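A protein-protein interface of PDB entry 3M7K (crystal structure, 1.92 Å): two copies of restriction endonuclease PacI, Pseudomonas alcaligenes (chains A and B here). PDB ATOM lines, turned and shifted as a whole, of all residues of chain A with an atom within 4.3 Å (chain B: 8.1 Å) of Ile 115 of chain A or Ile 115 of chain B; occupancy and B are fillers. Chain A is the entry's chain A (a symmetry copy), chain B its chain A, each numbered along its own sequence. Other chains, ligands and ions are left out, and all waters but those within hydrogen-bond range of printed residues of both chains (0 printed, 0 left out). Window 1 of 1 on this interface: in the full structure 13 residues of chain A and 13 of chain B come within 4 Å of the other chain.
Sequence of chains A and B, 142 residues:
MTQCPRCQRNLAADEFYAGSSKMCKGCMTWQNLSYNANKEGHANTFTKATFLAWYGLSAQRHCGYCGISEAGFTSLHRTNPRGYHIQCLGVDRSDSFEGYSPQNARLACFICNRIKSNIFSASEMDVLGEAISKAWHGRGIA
SG of Cys 109 of chain B lies close to N of Ile 111 of chain B (3.7 Å).
Among the printed residues, merely in contact across the chains: Ile 111 of chain A with Phe 120 of chain B (3.998 Å), Ile 115 of chain A with Ile 115 of chain B (3.9 Å), Ile 115 of chain A with Phe 120 of chain B (3.8 Å), Phe 120 of chain A with Ile 111 of chain B (3.999 Å), Phe 120 of chain A with Ile 115 of chain B (3.8 Å), Phe 120 of chain A with Trp 136 of chain B (3.9 Å), Leu 128 of chain A with Ile 132 of chain B (3.9 Å) and Ile 132 of chain A with Leu 128 of chain B (3.9 Å).
Ser 117 of chain A touches none of the printed residues of chain B. Printed residues of chain A within 4 Å of Ile 111 of chain B: Phe 120. Arg 114 of chain B touches none of the printed residues of chain A. Ile 115 of chain B touches just these residues of chain A: Ile 115 and Phe 120. Of the printed residues of chain A, Phe 120 of chain B touches Ile 111 (3.998 Å) and Ile 115 (3.8 Å).
Printed residues of chain B that touch a printed residue of chain A: Ile 111, Ile 115, Phe 120, Leu 128, Ile 132 and Trp 136. Hydrophobic or aromatic side chains of chain B within 4 Å of the printed part of chain A: Ile 111, Ile 115, Phe 120, Leu 128, Ile 132 and Trp 136. Hydrophobic or aromatic side chains of chain A within 4 Å of the printed part of chain B: Ile 111, Ile 115, Phe 120, Leu 128 and Ile 132. Along chain A the printed residues that touch a printed residue of chain B span positions 111 to 132. Among the printed residues, 8 pairs touch across the chains.
Ile 111 of chain A touches Phe 120 of chain B, and with the chains exchanged Phe 120 of chain A touches Ile 111 of chain B. Ile 115 of chain B touches its own counterpart, Ile 115 of chain A. Ile 115 of chain A touches Phe 120 of chain B, and with the chains exchanged Phe 120 of chain A touches Ile 115 of chain B. Leu 128 of chain A touches Ile 132 of chain B, and with the chains exchanged Ile 132 of chain A touches Leu 128 of chain B. Positions printed for both chains: 111, 112, 113, 114, 115, 116, 117, 120, 125, 128 and 132. Of the 8 pairs that touch across the chains among the printed residues, 7 have their exchanged pair printed and touching as well.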
ATOM      1  N   ILE A 111     -12.308   9.457  -2.900  1.00  0.00           N
ATOM      2  CA  ILE A 111     -13.384  10.245  -3.521  1.00  0.00           C
ATOM      3  C   ILE A 111     -13.094  11.749  -3.383  1.00  0.00           C
ATOM      4  O   ILE A 111     -13.118  12.478  -4.377  1.00  0.00           O
ATOM      5  CB  ILE A 111     -14.803   9.846  -3.004  1.00  0.00           C
ATOM      6  CG1 ILE A 111     -15.203   8.486  -3.595  1.00  0.00           C
ATOM      7  CG2 ILE A 111     -15.840  10.929  -3.360  1.00  0.00           C
ATOM      8  CD1 ILE A 111     -16.552   7.882  -3.088  1.00  0.00           C
ATOM      9  N   CYS A 112     -12.818  12.218  -2.163  1.00  0.00           N
ATOM     10  CA  CYS A 112     -12.566  13.646  -1.971  1.00  0.00           C
ATOM     11  C   CYS A 112     -11.253  14.060  -2.625  1.00  0.00           C
ATOM     12  O   CYS A 112     -11.131  15.162  -3.162  1.00  0.00           O
ATOM     13  CB  CYS A 112     -12.515  13.994  -0.477  1.00  0.00           C
ATOM     14  SG  CYS A 112     -14.134  13.902   0.307  1.00  0.00           S
ATOM     15  N   ASN A 113     -10.256  13.186  -2.565  1.00  0.00           N
ATOM     16  CA  ASN A 113      -8.963  13.510  -3.168  1.00  0.00           C
ATOM     17  C   ASN A 113      -9.136  13.798  -4.664  1.00  0.00           C
ATOM     18  O   ASN A 113      -8.570  14.777  -5.193  1.00  0.00           O
ATOM     19  CB  ASN A 113      -7.916  12.380  -2.932  1.00  0.00           C
ATOM     20  CG  ASN A 113      -6.523  12.939  -2.606  1.00  0.00           C
ATOM     21  OD1 ASN A 113      -6.275  14.153  -2.733  1.00  0.00           O
ATOM     22  ND2 ASN A 113      -5.626  12.075  -2.173  1.00  0.00           N
ATOM     23  N   ARG A 114      -9.884  12.929  -5.357  1.00  0.00           N
ATOM     24  CA  ARG A 114     -10.098  13.103  -6.809  1.00  0.00           C
ATOM     25  C   ARG A 114     -10.973  14.311  -7.099  1.00  0.00           C
ATOM     26  O   ARG A 114     -10.740  15.036  -8.077  1.00  0.00           O
ATOM     27  CB  ARG A 114     -10.740  11.870  -7.421  1.00  0.00           C
ATOM     28  CG  ARG A 114      -9.689  10.797  -7.704  1.00  0.00           C
ATOM     29  CD  ARG A 114     -10.248   9.888  -8.712  1.00  0.00           C
ATOM     30  NE  ARG A 114      -9.308   8.978  -9.326  1.00  0.00           N
ATOM     31  CZ  ARG A 114      -9.620   7.705  -9.590  1.00  0.00           C
ATOM     32  NH1 ARG A 114     -10.796   7.228  -9.194  1.00  0.00           N
ATOM     33  NH2 ARG A 114      -8.764   6.899 -10.221  1.00  0.00           N
ATOM     34  N   ILE A 115     -11.992  14.517  -6.272  1.00  0.00           N
ATOM     35  CA  ILE A 115     -12.854  15.711  -6.441  1.00  0.00           C
ATOM     36  C   ILE A 115     -12.080  17.017  -6.350  1.00  0.00           C
ATOM     37  O   ILE A 115     -12.166  17.881  -7.254  1.00  0.00           O
ATOM     38  CB  ILE A 115     -14.059  15.664  -5.464  1.00  0.00           C
ATOM     39  CG1 ILE A 115     -14.979  14.518  -5.913  1.00  0.00           C
ATOM     40  CG2 ILE A 115     -14.810  17.020  -5.437  1.00  0.00           C
ATOM     41  CD1 ILE A 115     -16.122  14.187  -4.932  1.00  0.00           C
ATOM     42  N   LYS A 116     -11.312  17.154  -5.273  1.00  0.00           N
ATOM     43  CA  LYS A 116     -10.500  18.335  -5.048  1.00  0.00           C
ATOM     44  C   LYS A 116      -9.542  18.505  -6.234  1.00  0.00           C
ATOM     45  O   LYS A 116      -9.383  19.629  -6.743  1.00  0.00           O
ATOM     46  CB  LYS A 116      -9.717  18.204  -3.729  1.00  0.00           C
ATOM     47  CG  LYS A 116      -8.832  19.412  -3.380  1.00  0.00           C
ATOM     48  CD  LYS A 116      -8.176  19.236  -1.974  1.00  0.00           C
ATOM     49  CE  LYS A 116      -7.027  20.245  -1.742  1.00  0.00           C
ATOM     50  NZ  LYS A 116      -5.733  19.822  -2.400  1.00  0.00           N
ATOM     51  N   SER A 117      -8.943  17.389  -6.676  1.00  0.00           N
ATOM     52  CA  SER A 117      -8.027  17.362  -7.822  1.00  0.00           C
ATOM     53  C   SER A 117      -7.024  18.515  -7.644  1.00  0.00           C
ATOM     54  O   SER A 117      -6.483  18.677  -6.550  1.00  0.00           O
ATOM     55  CB  SER A 117      -8.778  17.495  -9.160  1.00  0.00           C
ATOM     56  OG  SER A 117      -7.887  17.326 -10.272  1.00  0.00           O
ATOM     57  N   PHE A 120      -9.778  22.804  -6.577  1.00  0.00           N
ATOM     58  CA  PHE A 120     -10.262  23.518  -5.374  1.00  0.00           C
ATOM     59  C   PHE A 120      -9.173  23.684  -4.326  1.00  0.00           C
ATOM     60  O   PHE A 120      -8.335  22.795  -4.149  1.00  0.00           O
ATOM     61  CB  PHE A 120     -11.469  22.766  -4.754  1.00  0.00           C
ATOM     62  CG  PHE A 120     -12.659  22.653  -5.685  1.00  0.00           C
ATOM     63  CD1 PHE A 120     -12.931  21.470  -6.354  1.00  0.00           C
ATOM     64  CD2 PHE A 120     -13.466  23.764  -5.934  1.00  0.00           C
ATOM     65  CE1 PHE A 120     -14.016  21.364  -7.241  1.00  0.00           C
ATOM     66  CE2 PHE A 120     -14.551  23.688  -6.812  1.00  0.00           C
ATOM     67  CZ  PHE A 120     -14.834  22.474  -7.474  1.00  0.00           C
ATOM     68  N   MET A 125     -12.515  23.068  -0.546  1.00  0.00           N
ATOM     69  CA  MET A 125     -12.832  21.643  -0.407  1.00  0.00           C
ATOM     70  C   MET A 125     -13.450  21.302   0.961  1.00  0.00           C
ATOM     71  O   MET A 125     -14.246  20.343   1.075  1.00  0.00           O
ATOM     72  CB  MET A 125     -11.605  20.759  -0.691  1.00  0.00           C
ATOM     73  CG  MET A 125     -11.977  19.276  -0.853  1.00  0.00           C
ATOM     74  SD  MET A 125     -13.039  18.932  -2.306  1.00  0.00           S
ATOM     75  CE  MET A 125     -13.744  17.323  -1.879  1.00  0.00           C
ATOM     76  N   LEU A 128     -17.064  21.643   0.112  1.00  0.00           N
ATOM     77  CA  LEU A 128     -17.526  20.457  -0.622  1.00  0.00           C
ATOM     78  C   LEU A 128     -17.613  19.239   0.302  1.00  0.00           C
ATOM     79  O   LEU A 128     -18.564  18.454   0.220  1.00  0.00           O
ATOM     80  CB  LEU A 128     -16.605  20.132  -1.813  1.00  0.00           C
ATOM     81  CG  LEU A 128     -16.830  20.922  -3.102  1.00  0.00           C
ATOM     82  CD1 LEU A 128     -16.437  22.388  -2.946  1.00  0.00           C
ATOM     83  CD2 LEU A 128     -16.058  20.308  -4.248  1.00  0.00           C
ATOM     84  N   ILE A 132     -20.504  16.414   0.849  1.00  0.00           N
ATOM     85  CA  ILE A 132     -20.248  14.990   0.647  1.00  0.00           C
ATOM     86  C   ILE A 132     -20.607  14.188   1.907  1.00  0.00           C
ATOM     87  O   ILE A 132     -21.199  13.120   1.807  1.00  0.00           O
ATOM     88  CB  ILE A 132     -18.769  14.739   0.227  1.00  0.00           C
ATOM     89  CG1 ILE A 132     -18.497  15.363  -1.149  1.00  0.00           C
ATOM     90  CG2 ILE A 132     -18.448  13.239   0.190  1.00  0.00           C
ATOM     91  CD1 ILE A 132     -17.017  15.607  -1.444  1.00  0.00           C
ATOM     92  N   ARG B  78     -10.715  25.653 -18.239  1.00  0.00           N
ATOM     93  CA  ARG B  78     -10.579  24.221 -18.062  1.00  0.00           C
ATOM     94  C   ARG B  78     -10.249  23.607 -19.414  1.00  0.00           C
ATOM     95  O   ARG B  78     -10.656  24.147 -20.437  1.00  0.00           O
ATOM     96  CB  ARG B  78     -11.911  23.653 -17.573  1.00  0.00           C
ATOM     97  CG  ARG B  78     -12.414  24.279 -16.272  1.00  0.00           C
ATOM     98  CD  ARG B  78     -11.347  24.176 -15.184  1.00  0.00           C
ATOM     99  NE  ARG B  78     -11.025  22.778 -14.942  1.00  0.00           N
ATOM    100  CZ  ARG B  78      -9.994  22.339 -14.228  1.00  0.00           C
ATOM    101  NH1 ARG B  78      -9.804  21.027 -14.089  1.00  0.00           N
ATOM    102  NH2 ARG B  78      -9.156  23.192 -13.659  1.00  0.00           N
ATOM    103  N   CYS B 109     -21.764  21.704 -16.099  1.00  0.00           N
ATOM    104  CA  CYS B 109     -20.412  22.078 -16.479  1.00  0.00           C
ATOM    105  C   CYS B 109     -19.534  20.845 -16.306  1.00  0.00           C
ATOM    106  O   CYS B 109     -19.893  19.897 -15.570  1.00  0.00           O
ATOM    107  CB  CYS B 109     -19.880  23.256 -15.620  1.00  0.00           C
ATOM    108  SG  CYS B 109     -19.402  22.862 -13.871  1.00  0.00           S
ATOM    109  N   PHE B 110     -18.408  20.816 -16.995  1.00  0.00           N
ATOM    110  CA  PHE B 110     -17.552  19.620 -16.977  1.00  0.00           C
ATOM    111  C   PHE B 110     -16.970  19.326 -15.592  1.00  0.00           C
ATOM    112  O   PHE B 110     -16.663  18.160 -15.267  1.00  0.00           O
ATOM    113  CB  PHE B 110     -16.433  19.766 -18.011  1.00  0.00           C
ATOM    114  CG  PHE B 110     -15.775  18.457 -18.415  1.00  0.00           C
ATOM    115  CD1 PHE B 110     -16.521  17.282 -18.542  1.00  0.00           C
ATOM    116  CD2 PHE B 110     -14.403  18.418 -18.701  1.00  0.00           C
ATOM    117  CE1 PHE B 110     -15.924  16.087 -18.910  1.00  0.00           C
ATOM    118  CE2 PHE B 110     -13.784  17.224 -19.122  1.00  0.00           C
ATOM    119  CZ  PHE B 110     -14.547  16.050 -19.229  1.00  0.00           C
ATOM    120  N   ILE B 111     -16.822  20.366 -14.767  1.00  0.00           N
ATOM    121  CA  ILE B 111     -16.363  20.149 -13.385  1.00  0.00           C
ATOM    122  C   ILE B 111     -17.408  19.342 -12.596  1.00  0.00           C
ATOM    123  O   ILE B 111     -17.072  18.325 -11.986  1.00  0.00           O
ATOM    124  CB  ILE B 111     -15.947  21.473 -12.671  1.00  0.00           C
ATOM    125  CG1 ILE B 111     -14.606  21.964 -13.237  1.00  0.00           C
ATOM    126  CG2 ILE B 111     -15.860  21.269 -11.146  1.00  0.00           C
ATOM    127  CD1 ILE B 111     -14.097  23.344 -12.710  1.00  0.00           C
ATOM    128  N   CYS B 112     -18.669  19.783 -12.606  1.00  0.00           N
ATOM    129  CA  CYS B 112     -19.695  19.070 -11.845  1.00  0.00           C
ATOM    130  C   CYS B 112     -19.977  17.704 -12.458  1.00  0.00           C
ATOM    131  O   CYS B 112     -20.240  16.732 -11.749  1.00  0.00           O
ATOM    132  CB  CYS B 112     -20.999  19.880 -11.799  1.00  0.00           C
ATOM    133  SG  CYS B 112     -20.864  21.343 -10.757  1.00  0.00           S
ATOM    134  N   ASN B 113     -19.946  17.628 -13.783  1.00  0.00           N
ATOM    135  CA  ASN B 113     -20.208  16.351 -14.448  1.00  0.00           C
ATOM    136  C   ASN B 113     -19.203  15.295 -13.975  1.00  0.00           C
ATOM    137  O   ASN B 113     -19.584  14.144 -13.674  1.00  0.00           O
ATOM    138  CB  ASN B 113     -20.185  16.493 -15.999  1.00  0.00           C
ATOM    139  CG  ASN B 113     -21.295  15.673 -16.673  1.00  0.00           C
ATOM    140  OD1 ASN B 113     -21.969  14.852 -16.022  1.00  0.00           O
ATOM    141  ND2 ASN B 113     -21.501  15.898 -17.956  1.00  0.00           N
ATOM    142  N   ARG B 114     -17.916  15.666 -13.944  1.00  0.00           N
ATOM    143  CA  ARG B 114     -16.863  14.717 -13.524  1.00  0.00           C
ATOM    144  C   ARG B 114     -16.960  14.406 -12.039  1.00  0.00           C
ATOM    145  O   ARG B 114     -16.738  13.261 -11.621  1.00  0.00           O
ATOM    146  CB  ARG B 114     -15.478  15.264 -13.825  1.00  0.00           C
ATOM    147  CG  ARG B 114     -15.109  15.024 -15.289  1.00  0.00           C
ATOM    148  CD  ARG B 114     -13.646  15.099 -15.392  1.00  0.00           C
ATOM    149  NE  ARG B 114     -13.080  14.617 -16.630  1.00  0.00           N
ATOM    150  CZ  ARG B 114     -12.062  15.237 -17.235  1.00  0.00           C
ATOM    151  NH1 ARG B 114     -11.612  16.385 -16.737  1.00  0.00           N
ATOM    152  NH2 ARG B 114     -11.505  14.738 -18.340  1.00  0.00           N
ATOM    153  N   ILE B 115     -17.264  15.423 -11.240  1.00  0.00           N
ATOM    154  CA  ILE B 115     -17.446  15.193  -9.786  1.00  0.00           C
ATOM    155  C   ILE B 115     -18.543  14.186  -9.480  1.00  0.00           C
ATOM    156  O   ILE B 115     -18.322  13.197  -8.742  1.00  0.00           O
ATOM    157  CB  ILE B 115     -17.646  16.537  -9.037  1.00  0.00           C
ATOM    158  CG1 ILE B 115     -16.315  17.304  -9.093  1.00  0.00           C
ATOM    159  CG2 ILE B 115     -18.105  16.300  -7.576  1.00  0.00           C
ATOM    160  CD1 ILE B 115     -16.386  18.757  -8.580  1.00  0.00           C
ATOM    161  N   LYS B 116     -19.718  14.424 -10.058  1.00  0.00           N
ATOM    162  CA  LYS B 116     -20.860  13.548  -9.876  1.00  0.00           C
ATOM    163  C   LYS B 116     -20.475  12.138 -10.342  1.00  0.00           C
ATOM    164  O   LYS B 116     -20.785  11.153  -9.647  1.00  0.00           O
ATOM    165  CB  LYS B 116     -22.069  14.073 -10.670  1.00  0.00           C
ATOM    166  CG  LYS B 116     -23.346  13.227 -10.538  1.00  0.00           C
ATOM    167  CD  LYS B 116     -24.543  13.903 -11.278  1.00  0.00           C
ATOM    168  CE  LYS B 116     -25.733  12.932 -11.461  1.00  0.00           C
ATOM    169  NZ  LYS B 116     -25.545  11.986 -12.625  1.00  0.00           N
ATOM    170  N   SER B 117     -19.782  12.060 -11.488  1.00  0.00           N
ATOM    171  CA  SER B 117     -19.302  10.797 -12.059  1.00  0.00           C
ATOM    172  C   SER B 117     -20.472   9.799 -12.031  1.00  0.00           C
ATOM    173  O   SER B 117     -21.580  10.160 -12.428  1.00  0.00           O
ATOM    174  CB  SER B 117     -18.093  10.241 -11.285  1.00  0.00           C
ATOM    175  OG  SER B 117     -17.548   9.084 -11.937  1.00  0.00           O
ATOM    176  N   ASN B 118     -20.232   8.568 -11.577  1.00  0.00           N
ATOM    177  CA  ASN B 118     -21.336   7.654 -11.281  1.00  0.00           C
ATOM    178  C   ASN B 118     -21.418   7.380  -9.785  1.00  0.00           C
ATOM    179  O   ASN B 118     -21.983   6.378  -9.353  1.00  0.00           O
ATOM    180  CB  ASN B 118     -21.228   6.338 -12.070  1.00  0.00           C
ATOM    181  CG  ASN B 118     -20.055   5.474 -11.619  1.00  0.00           C
ATOM    182  OD1 ASN B 118     -19.120   5.947 -10.958  1.00  0.00           O
ATOM    183  ND2 ASN B 118     -20.083   4.198 -12.007  1.00  0.00           N
ATOM    184  N   ILE B 119     -20.883   8.296  -8.999  1.00  0.00           N
ATOM    185  CA  ILE B 119     -20.843   8.151  -7.546  1.00  0.00           C
ATOM    186  C   ILE B 119     -22.126   8.675  -6.909  1.00  0.00           C
ATOM    187  O   ILE B 119     -22.781   7.957  -6.142  1.00  0.00           O
ATOM    188  CB  ILE B 119     -19.639   8.951  -6.965  1.00  0.00           C
ATOM    189  CG1 ILE B 119     -18.323   8.378  -7.474  1.00  0.00           C
ATOM    190  CG2 ILE B 119     -19.645   8.916  -5.432  1.00  0.00           C
ATOM    191  CD1 ILE B 119     -17.106   9.299  -7.193  1.00  0.00           C
ATOM    192  N   PHE B 120     -22.489   9.917  -7.232  1.00  0.00           N
ATOM    193  CA  PHE B 120     -23.563  10.643  -6.519  1.00  0.00           C
ATOM    194  C   PHE B 120     -24.863  10.671  -7.309  1.00  0.00           C
ATOM    195  O   PHE B 120     -24.843  10.769  -8.539  1.00  0.00           O
ATOM    196  CB  PHE B 120     -23.114  12.095  -6.207  1.00  0.00           C
ATOM    197  CG  PHE B 120     -21.889  12.176  -5.320  1.00  0.00           C
ATOM    198  CD1 PHE B 120     -20.640  12.456  -5.851  1.00  0.00           C
ATOM    199  CD2 PHE B 120     -21.990  11.903  -3.954  1.00  0.00           C
ATOM    200  CE1 PHE B 120     -19.493  12.506  -5.040  1.00  0.00           C
ATOM    201  CE2 PHE B 120     -20.865  11.944  -3.124  1.00  0.00           C
ATOM    202  CZ  PHE B 120     -19.601  12.250  -3.670  1.00  0.00           C
ATOM    203  N   MET B 125     -25.931  15.361  -5.666  1.00  0.00           N
ATOM    204  CA  MET B 125     -25.121  16.332  -6.410  1.00  0.00           C
ATOM    205  C   MET B 125     -25.683  17.762  -6.328  1.00  0.00           C
ATOM    206  O   MET B 125     -24.917  18.749  -6.405  1.00  0.00           O
ATOM    207  CB  MET B 125     -24.926  15.902  -7.875  1.00  0.00           C
ATOM    208  CG  MET B 125     -23.842  16.727  -8.588  1.00  0.00           C
ATOM    209  SD  MET B 125     -22.160  16.499  -7.896  1.00  0.00           S
ATOM    210  CE  MET B 125     -21.304  17.967  -8.510  1.00  0.00           C
ATOM    211  N   LEU B 128     -23.783  19.005  -3.371  1.00  0.00           N
ATOM    212  CA  LEU B 128     -22.409  19.348  -3.759  1.00  0.00           C
ATOM    213  C   LEU B 128     -22.380  20.620  -4.612  1.00  0.00           C
ATOM    214  O   LEU B 128     -21.503  21.473  -4.438  1.00  0.00           O
ATOM    215  CB  LEU B 128     -21.733  18.199  -4.531  1.00  0.00           C
ATOM    216  CG  LEU B 128     -21.133  17.062  -3.702  1.00  0.00           C
ATOM    217  CD1 LEU B 128     -22.212  16.229  -3.016  1.00  0.00           C
ATOM    218  CD2 LEU B 128     -20.272  16.168  -4.565  1.00  0.00           C
ATOM    219  N   GLY B 129     -23.319  20.724  -5.549  1.00  0.00           N
ATOM    220  CA  GLY B 129     -23.432  21.919  -6.404  1.00  0.00           C
ATOM    221  C   GLY B 129     -23.491  23.248  -5.648  1.00  0.00           C
ATOM    222  O   GLY B 129     -22.803  24.211  -6.038  1.00  0.00           O
ATOM    223  N   ILE B 132     -20.055  23.968  -4.462  1.00  0.00           N
ATOM    224  CA  ILE B 132     -19.230  24.393  -5.590  1.00  0.00           C
ATOM    225  C   ILE B 132     -19.564  25.836  -5.997  1.00  0.00           C
ATOM    226  O   ILE B 132     -18.664  26.619  -6.274  1.00  0.00           O
ATOM    227  CB  ILE B 132     -19.385  23.422  -6.797  1.00  0.00           C
ATOM    228  CG1 ILE B 132     -18.833  22.035  -6.435  1.00  0.00           C
ATOM    229  CG2 ILE B 132     -18.664  23.959  -8.041  1.00  0.00           C
ATOM    230  CD1 ILE B 132     -19.351  20.903  -7.322  1.00  0.00           C
ATOM    231  N   TRP B 136     -17.217  29.352  -6.486  1.00  0.00           N
ATOM    232  CA  TRP B 136     -17.250  30.295  -7.610  1.00  0.00           C
ATOM    233  C   TRP B 136     -17.551  31.711  -7.106  1.00  0.00           C
ATOM    234  O   TRP B 136     -16.811  32.652  -7.424  1.00  0.00           O
ATOM    235  CB  TRP B 136     -18.277  29.891  -8.674  1.00  0.00           C
ATOM    236  CG  TRP B 136     -18.152  28.468  -9.279  1.00  0.00           C
ATOM    237  CD1 TRP B 136     -19.181  27.713  -9.764  1.00  0.00           C
ATOM    238  CD2 TRP B 136     -16.961  27.678  -9.460  1.00  0.00           C
ATOM    239  NE1 TRP B 136     -18.715  26.512 -10.227  1.00  0.00           N
ATOM    240  CE2 TRP B 136     -17.360  26.456 -10.056  1.00  0.00           C
ATOM    241  CE3 TRP B 136     -15.605  27.878  -9.175  1.00  0.00           C
ATOM    242  CZ2 TRP B 136     -16.447  25.425 -10.371  1.00  0.00           C
ATOM    243  CZ3 TRP B 136     -14.693  26.865  -9.489  1.00  0.00           C
ATOM    244  CH2 TRP B 136     -15.121  25.648 -10.080  1.00  0.00           C
